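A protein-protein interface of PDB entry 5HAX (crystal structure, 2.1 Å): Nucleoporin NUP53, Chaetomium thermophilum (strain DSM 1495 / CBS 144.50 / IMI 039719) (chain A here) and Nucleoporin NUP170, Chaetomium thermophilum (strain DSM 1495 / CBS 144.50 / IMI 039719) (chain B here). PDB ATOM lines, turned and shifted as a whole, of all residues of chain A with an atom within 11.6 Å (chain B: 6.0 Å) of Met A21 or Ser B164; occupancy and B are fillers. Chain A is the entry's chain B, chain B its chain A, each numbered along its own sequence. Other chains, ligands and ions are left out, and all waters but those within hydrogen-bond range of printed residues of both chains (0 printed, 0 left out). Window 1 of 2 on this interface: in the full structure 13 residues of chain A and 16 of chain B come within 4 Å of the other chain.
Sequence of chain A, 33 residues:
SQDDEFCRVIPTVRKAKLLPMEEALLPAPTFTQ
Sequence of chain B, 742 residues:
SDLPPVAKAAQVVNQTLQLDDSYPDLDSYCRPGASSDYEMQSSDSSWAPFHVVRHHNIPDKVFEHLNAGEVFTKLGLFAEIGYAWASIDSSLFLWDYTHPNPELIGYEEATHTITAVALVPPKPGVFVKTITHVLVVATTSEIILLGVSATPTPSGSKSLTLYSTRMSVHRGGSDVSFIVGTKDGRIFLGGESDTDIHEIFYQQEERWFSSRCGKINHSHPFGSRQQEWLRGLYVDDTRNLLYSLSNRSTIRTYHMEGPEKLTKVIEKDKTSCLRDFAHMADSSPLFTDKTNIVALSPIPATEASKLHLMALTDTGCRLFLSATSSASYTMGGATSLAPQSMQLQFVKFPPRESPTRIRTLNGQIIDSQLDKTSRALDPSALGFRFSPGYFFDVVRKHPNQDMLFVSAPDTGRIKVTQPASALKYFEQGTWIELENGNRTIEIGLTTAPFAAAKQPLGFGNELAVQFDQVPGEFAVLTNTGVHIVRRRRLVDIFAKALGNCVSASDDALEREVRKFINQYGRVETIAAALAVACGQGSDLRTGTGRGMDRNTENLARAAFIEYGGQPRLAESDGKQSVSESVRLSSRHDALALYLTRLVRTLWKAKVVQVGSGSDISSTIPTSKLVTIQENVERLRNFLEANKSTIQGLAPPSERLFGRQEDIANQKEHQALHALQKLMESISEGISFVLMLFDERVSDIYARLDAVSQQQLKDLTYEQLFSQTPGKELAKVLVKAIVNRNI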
ATOM      1  N   ALA A  16       3.642 -29.471   7.318  1.00  0.00           N
ATOM      2  CA  ALA A  16       2.896 -28.510   8.119  1.00  0.00           C
ATOM      3  C   ALA A  16       3.751 -27.967   9.258  1.00  0.00           C
ATOM      4  O   ALA A  16       4.408 -28.726   9.978  1.00  0.00           O
ATOM      5  CB  ALA A  16       1.631 -29.162   8.677  1.00  0.00           C
ATOM      6  N   LYS A  17       3.738 -26.645   9.413  1.00  0.00           N
ATOM      7  CA  LYS A  17       4.431 -25.994  10.518  1.00  0.00           C
ATOM      8  C   LYS A  17       3.732 -26.337  11.829  1.00  0.00           C
ATOM      9  O   LYS A  17       2.548 -26.034  12.003  1.00  0.00           O
ATOM     10  CB  LYS A  17       4.451 -24.484  10.295  1.00  0.00           C
ATOM     11  CG  LYS A  17       5.110 -23.664  11.398  1.00  0.00           C
ATOM     12  CD  LYS A  17       4.425 -22.310  11.528  1.00  0.00           C
ATOM     13  CE  LYS A  17       5.358 -21.244  12.075  1.00  0.00           C
ATOM     14  NZ  LYS A  17       4.710 -19.903  12.057  1.00  0.00           N
ATOM     15  N   LEU A  18       4.464 -26.964  12.750  1.00  0.00           N
ATOM     16  CA  LEU A  18       3.929 -27.355  14.053  1.00  0.00           C
ATOM     17  C   LEU A  18       4.348 -26.301  15.074  1.00  0.00           C
ATOM     18  O   LEU A  18       5.496 -26.276  15.524  1.00  0.00           O
ATOM     19  CB  LEU A  18       4.423 -28.741  14.453  1.00  0.00           C
ATOM     20  CG  LEU A  18       4.223 -29.870  13.440  1.00  0.00           C
ATOM     21  CD1 LEU A  18       4.958 -31.114  13.909  1.00  0.00           C
ATOM     22  CD2 LEU A  18       2.745 -30.170  13.225  1.00  0.00           C
ATOM     23  N   LEU A  19       3.410 -25.429  15.437  1.00  0.00           N
ATOM     24  CA  LEU A  19       3.679 -24.400  16.426  1.00  0.00           C
ATOM     25  C   LEU A  19       3.953 -25.037  17.788  1.00  0.00           C
ATOM     26  O   LEU A  19       3.544 -26.171  18.047  1.00  0.00           O
ATOM     27  CB  LEU A  19       2.502 -23.432  16.502  1.00  0.00           C
ATOM     28  CG  LEU A  19       2.229 -22.635  15.224  1.00  0.00           C
ATOM     29  CD1 LEU A  19       0.941 -21.840  15.362  1.00  0.00           C
ATOM     30  CD2 LEU A  19       3.394 -21.712  14.894  1.00  0.00           C
ATOM     31  N   PRO A  20       4.640 -24.325  18.679  1.00  0.00           N
ATOM     32  CA  PRO A  20       5.201 -24.978  19.866  1.00  0.00           C
ATOM     33  C   PRO A  20       4.150 -25.328  20.907  1.00  0.00           C
ATOM     34  O   PRO A  20       3.020 -24.831  20.904  1.00  0.00           O
ATOM     35  CB  PRO A  20       6.186 -23.939  20.407  1.00  0.00           C
ATOM     36  CG  PRO A  20       5.615 -22.639  19.986  1.00  0.00           C
ATOM     37  CD  PRO A  20       4.951 -22.883  18.652  1.00  0.00           C
ATOM     38  N   MET A  21       4.561 -26.217  21.817  1.00  0.00           N
ATOM     39  CA  MET A  21       3.728 -26.591  22.955  1.00  0.00           C
ATOM     40  C   MET A  21       3.452 -25.399  23.861  1.00  0.00           C
ATOM     41  O   MET A  21       2.392 -25.335  24.495  1.00  0.00           O
ATOM     42  CB  MET A  21       4.424 -27.707  23.740  1.00  0.00           C
ATOM     43  CG  MET A  21       3.704 -28.189  24.995  1.00  0.00           C
ATOM     44  SD  MET A  21       4.861 -28.691  26.288  1.00  0.00           S
ATOM     45  CE  MET A  21       5.183 -27.114  27.079  1.00  0.00           C
ATOM     46  N   GLU A  22       4.389 -24.450  23.933  1.00  0.00           N
ATOM     47  CA  GLU A  22       4.251 -23.322  24.851  1.00  0.00           C
ATOM     48  C   GLU A  22       2.957 -22.561  24.600  1.00  0.00           C
ATOM     49  O   GLU A  22       2.230 -22.219  25.542  1.00  0.00           O
ATOM     50  CB  GLU A  22       5.458 -22.394  24.716  1.00  0.00           C
ATOM     51  CG  GLU A  22       6.695 -22.869  25.467  1.00  0.00           C
ATOM     52  CD  GLU A  22       7.269 -24.161  24.912  1.00  0.00           C
ATOM     53  OE1 GLU A  22       7.986 -24.860  25.659  1.00  0.00           O
ATOM     54  OE2 GLU A  22       7.012 -24.474  23.732  1.00  0.00           O
ATOM     55  N   GLU A  23       2.650 -22.280  23.333  1.00  0.00           N
ATOM     56  CA  GLU A  23       1.376 -21.649  23.006  1.00  0.00           C
ATOM     57  C   GLU A  23       0.213 -22.589  23.291  1.00  0.00           C
ATOM     58  O   GLU A  23      -0.769 -22.199  23.934  1.00  0.00           O
ATOM     59  CB  GLU A  23       1.366 -21.216  21.539  1.00  0.00           C
ATOM     60  CG  GLU A  23      -0.028 -20.924  20.992  1.00  0.00           C
ATOM     61  CD  GLU A  23      -0.048 -19.798  19.976  1.00  0.00           C
ATOM     62  OE1 GLU A  23       1.011 -19.501  19.381  1.00  0.00           O
ATOM     63  OE2 GLU A  23      -1.129 -19.205  19.777  1.00  0.00           O
ATOM     64  N   ALA A  24       0.311 -23.831  22.817  1.00  0.00           N
ATOM     65  CA  ALA A  24      -0.745 -24.828  22.950  1.00  0.00           C
ATOM     66  C   ALA A  24      -1.317 -24.901  24.360  1.00  0.00           C
ATOM     67  O   ALA A  24      -2.459 -24.493  24.583  1.00  0.00           O
ATOM     68  CB  ALA A  24      -0.223 -26.204  22.534  1.00  0.00           C
ATOM     69  N   LEU A  25      -0.553 -25.410  25.322  1.00  0.00           N
ATOM     70  CA  LEU A  25      -1.087 -25.629  26.658  1.00  0.00           C
ATOM     71  C   LEU A  25      -0.764 -24.465  27.581  1.00  0.00           C
ATOM     72  O   LEU A  25       0.343 -23.916  27.565  1.00  0.00           O
ATOM     73  CB  LEU A  25      -0.575 -26.937  27.262  1.00  0.00           C
ATOM     74  CG  LEU A  25       0.920 -27.132  27.485  1.00  0.00           C
ATOM     75  CD1 LEU A  25       1.332 -26.703  28.886  1.00  0.00           C
ATOM     76  CD2 LEU A  25       1.253 -28.593  27.246  1.00  0.00           C
ATOM     77  N   LEU A  26      -1.767 -24.089  28.364  1.00  0.00           N
ATOM     78  CA  LEU A  26      -1.670 -23.085  29.409  1.00  0.00           C
ATOM     79  C   LEU A  26      -1.178 -23.749  30.696  1.00  0.00           C
ATOM     80  O   LEU A  26      -1.084 -24.976  30.762  1.00  0.00           O
ATOM     81  CB  LEU A  26      -3.041 -22.420  29.615  1.00  0.00           C
ATOM     82  CG  LEU A  26      -4.201 -23.386  29.901  1.00  0.00           C
ATOM     83  CD1 LEU A  26      -4.232 -23.834  31.359  1.00  0.00           C
ATOM     84  CD2 LEU A  26      -5.540 -22.784  29.507  1.00  0.00           C
ATOM     85  N   PRO A  27      -0.859 -22.950  31.726  1.00  0.00           N
ATOM     86  CA  PRO A  27      -0.706 -21.493  31.728  1.00  0.00           C
ATOM     87  C   PRO A  27       0.762 -21.078  31.798  1.00  0.00           C
ATOM     88  O   PRO A  27       1.592 -21.902  32.193  1.00  0.00           O
ATOM     89  CB  PRO A  27      -1.463 -21.075  32.989  1.00  0.00           C
ATOM     90  CG  PRO A  27      -1.422 -22.299  33.903  1.00  0.00           C
ATOM     91  CD  PRO A  27      -0.888 -23.469  33.105  1.00  0.00           C
ATOM     92  N   LEU B 145      -0.569 -37.434  19.921  1.00  0.00           N
ATOM     93  CA  LEU B 145      -1.567 -36.381  20.056  1.00  0.00           C
ATOM     94  C   LEU B 145      -1.017 -35.084  19.478  1.00  0.00           C
ATOM     95  O   LEU B 145       0.116 -34.697  19.779  1.00  0.00           O
ATOM     96  CB  LEU B 145      -1.952 -36.171  21.520  1.00  0.00           C
ATOM     97  CG  LEU B 145      -2.430 -37.396  22.297  1.00  0.00           C
ATOM     98  CD1 LEU B 145      -2.791 -36.992  23.718  1.00  0.00           C
ATOM     99  CD2 LEU B 145      -3.611 -38.058  21.602  1.00  0.00           C
ATOM    100  N   LEU B 146      -1.825 -34.417  18.654  1.00  0.00           N
ATOM    101  CA  LEU B 146      -1.485 -33.114  18.102  1.00  0.00           C
ATOM    102  C   LEU B 146      -2.608 -32.133  18.393  1.00  0.00           C
ATOM    103  O   LEU B 146      -3.789 -32.464  18.248  1.00  0.00           O
ATOM    104  CB  LEU B 146      -1.248 -33.182  16.589  1.00  0.00           C
ATOM    105  CG  LEU B 146      -0.055 -34.006  16.105  1.00  0.00           C
ATOM    106  CD1 LEU B 146       0.025 -33.972  14.588  1.00  0.00           C
ATOM    107  CD2 LEU B 146       1.241 -33.500  16.716  1.00  0.00           C
ATOM    108  N   GLY B 147      -2.232 -30.929  18.812  1.00  0.00           N
ATOM    109  CA  GLY B 147      -3.209 -29.870  18.963  1.00  0.00           C
ATOM    110  C   GLY B 147      -3.683 -29.363  17.615  1.00  0.00           C
ATOM    111  O   GLY B 147      -2.931 -29.316  16.642  1.00  0.00           O
ATOM    112  N   LEU B 162      -1.698 -26.965  13.004  1.00  0.00           N
ATOM    113  CA  LEU B 162      -1.335 -28.049  13.905  1.00  0.00           C
ATOM    114  C   LEU B 162      -0.306 -27.583  14.927  1.00  0.00           C
ATOM    115  O   LEU B 162       0.554 -26.748  14.632  1.00  0.00           O
ATOM    116  CB  LEU B 162      -0.784 -29.240  13.118  1.00  0.00           C
ATOM    117  CG  LEU B 162      -1.744 -29.817  12.075  1.00  0.00           C
ATOM    118  CD1 LEU B 162      -1.028 -30.814  11.179  1.00  0.00           C
ATOM    119  CD2 LEU B 162      -2.942 -30.464  12.752  1.00  0.00           C
ATOM    120  N   TYR B 163      -0.405 -28.139  16.135  1.00  0.00           N
ATOM    121  CA  TYR B 163       0.487 -27.821  17.242  1.00  0.00           C
ATOM    122  C   TYR B 163       1.072 -29.103  17.811  1.00  0.00           C
ATOM    123  O   TYR B 163       0.353 -30.087  18.013  1.00  0.00           O
ATOM    124  CB  TYR B 163      -0.245 -27.069  18.361  1.00  0.00           C
ATOM    125  CG  TYR B 163      -0.805 -25.727  17.955  1.00  0.00           C
ATOM    126  CD1 TYR B 163      -0.218 -24.549  18.393  1.00  0.00           C
ATOM    127  CD2 TYR B 163      -1.927 -25.636  17.145  1.00  0.00           C
ATOM    128  CE1 TYR B 163      -0.725 -23.318  18.029  1.00  0.00           C
ATOM    129  CE2 TYR B 163      -2.444 -24.410  16.774  1.00  0.00           C
ATOM    130  CZ  TYR B 163      -1.840 -23.253  17.220  1.00  0.00           C
ATOM    131  OH  TYR B 163      -2.351 -22.030  16.853  1.00  0.00           O
ATOM    132  N   SER B 164       2.377 -29.088  18.076  1.00  0.00           N
ATOM    133  CA  SER B 164       3.003 -30.192  18.783  1.00  0.00           C
ATOM    134  C   SER B 164       2.629 -30.140  20.262  1.00  0.00           C
ATOM    135  O   SER B 164       2.200 -29.109  20.788  1.00  0.00           O
ATOM    136  CB  SER B 164       4.520 -30.151  18.615  1.00  0.00           C
ATOM    137  OG  SER B 164       5.059 -28.939  19.111  1.00  0.00           O
ATOM    138  N   THR B 165       2.790 -31.281  20.935  1.00  0.00           N
ATOM    139  CA  THR B 165       2.344 -31.426  22.319  1.00  0.00           C
ATOM    140  C   THR B 165       3.321 -32.162  23.219  1.00  0.00           C
ATOM    141  O   THR B 165       3.170 -32.076  24.443  1.00  0.00           O
ATOM    142  CB  THR B 165       0.999 -32.165  22.372  1.00  0.00           C
ATOM    143  OG1 THR B 165       1.183 -33.527  21.962  1.00  0.00           O
ATOM    144  CG2 THR B 165      -0.029 -31.497  21.473  1.00  0.00           C
ATOM    145  N   ARG B 166       4.304 -32.881  22.682  1.00  0.00           N
ATOM    146  CA  ARG B 166       5.166 -33.779  23.446  1.00  0.00           C
ATOM    147  C   ARG B 166       4.382 -34.903  24.112  1.00  0.00           C
ATOM    148  O   ARG B 166       4.929 -35.607  24.971  1.00  0.00           O
ATOM    149  CB  ARG B 166       5.980 -33.025  24.509  1.00  0.00           C
ATOM    150  CG  ARG B 166       6.753 -31.823  23.987  1.00  0.00           C
ATOM    151  CD  ARG B 166       7.550 -31.176  25.110  1.00  0.00           C
ATOM    152  NE  ARG B 166       7.946 -29.804  24.800  1.00  0.00           N
ATOM    153  CZ  ARG B 166       8.324 -28.912  25.709  1.00  0.00           C
ATOM    154  NH1 ARG B 166       8.353 -29.236  26.997  1.00  0.00           N
ATOM    155  NH2 ARG B 166       8.669 -27.686  25.334  1.00  0.00           N
ATOM    156  N   ARG B 212       3.343 -36.819  31.194  1.00  0.00           N
ATOM    157  CA  ARG B 212       2.269 -35.985  30.666  1.00  0.00           C
ATOM    158  C   ARG B 212       1.203 -36.791  29.939  1.00  0.00           C
ATOM    159  O   ARG B 212       0.090 -36.288  29.758  1.00  0.00           O
ATOM    160  CB  ARG B 212       2.828 -34.935  29.705  1.00  0.00           C
ATOM    161  CG  ARG B 212       3.143 -33.593  30.335  1.00  0.00           C
ATOM    162  CD  ARG B 212       2.970 -32.480  29.312  1.00  0.00           C
ATOM    163  NE  ARG B 212       3.425 -31.187  29.814  1.00  0.00           N
ATOM    164  CZ  ARG B 212       4.655 -30.706  29.658  1.00  0.00           C
ATOM    165  NH1 ARG B 212       4.965 -29.516  30.155  1.00  0.00           N
ATOM    166  NH2 ARG B 212       5.577 -31.407  29.011  1.00  0.00           N
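The backbone carbonyl oxygen (O) of Leu B162 sits at hydrogen-bond distance from the backbone NH (N) of Leu A19, at 3.2 Å.
N of Ser B164 sits at hydrogen-bond distance from O of Leu A19 (3.1 Å).
The side-chain sulfur (SD) of Met A21 sits close to the guanidinium group (NE) of Arg B166 (3.6 Å).
The guanidinium group of Arg B166 is in salt-bridge range of the side-chain carboxylate of Glu A22.
O of Lys A17 lies close to O of Leu B162, 3.4 Å away.
Printed residues of chain B within 4 Å of Lys A17: Leu B162.
Printed residues of chain B within 4 Å of Glu A22: Arg B166.
Printed residues of chain B within 4 Å of Glu A23: Tyr B163 (3.9 Å).
No residue of chain A comes within 4 Å of Gly B147.
Printed residues of chain A within 4 Å of Tyr B163: Leu A19 and Glu A23.
Of chain A, only Leu A19 and Met A21 come within 4 Å of Ser B164.
Of the printed residues of chain A, Arg B166 touches Met A21 (3.5 Å) and Glu A22 (2.9 Å).
The nearest printed residue of chain B that does not touch Met A21 is Tyr B163 (6.0 Å).
The nearest printed residue of chain A that does not touch Arg B212 is Leu A25 (4.2 Å).
Among the printed residues, pairs that only touch across the chains: Leu A18 with Leu B162, Leu A19 with Tyr B163, Met A21 with Ser B164, Met A21 with Thr B165, Met A21 with Arg B212 and Glu A23 with Tyr B163.
Of the 12 printed residues of chain A, 6 touch a printed residue of chain B.
Of the 9 printed residues of chain B, 6 touch a printed residue of chain A.
Printed residues of chain B that touch a printed residue of chain A: Leu B162, Tyr B163, Ser B164, Thr B165, Arg B166 and Arg B212.
Hydrophobic or aromatic side chains of chain B within 4 Å of the printed part of chain A: Leu B162 and Tyr B163.
Among the printed residues, 11 pairs touch across the chains.
Among the printed residues, Asp or Glu carboxylates within 4 Å of a Lys or Arg side-chain nitrogen of the other chain: Glu A22 with Arg B166 (2.9 Å).
OG1 of Thr B165 lies within hydrogen-bond range of O of Leu B145 (2.7 Å).
The backbone NH (N) of Tyr B163 is in hydrogen-bond range of the backbone carbonyl oxygen (O) of Gly B147 (2.8 Å).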
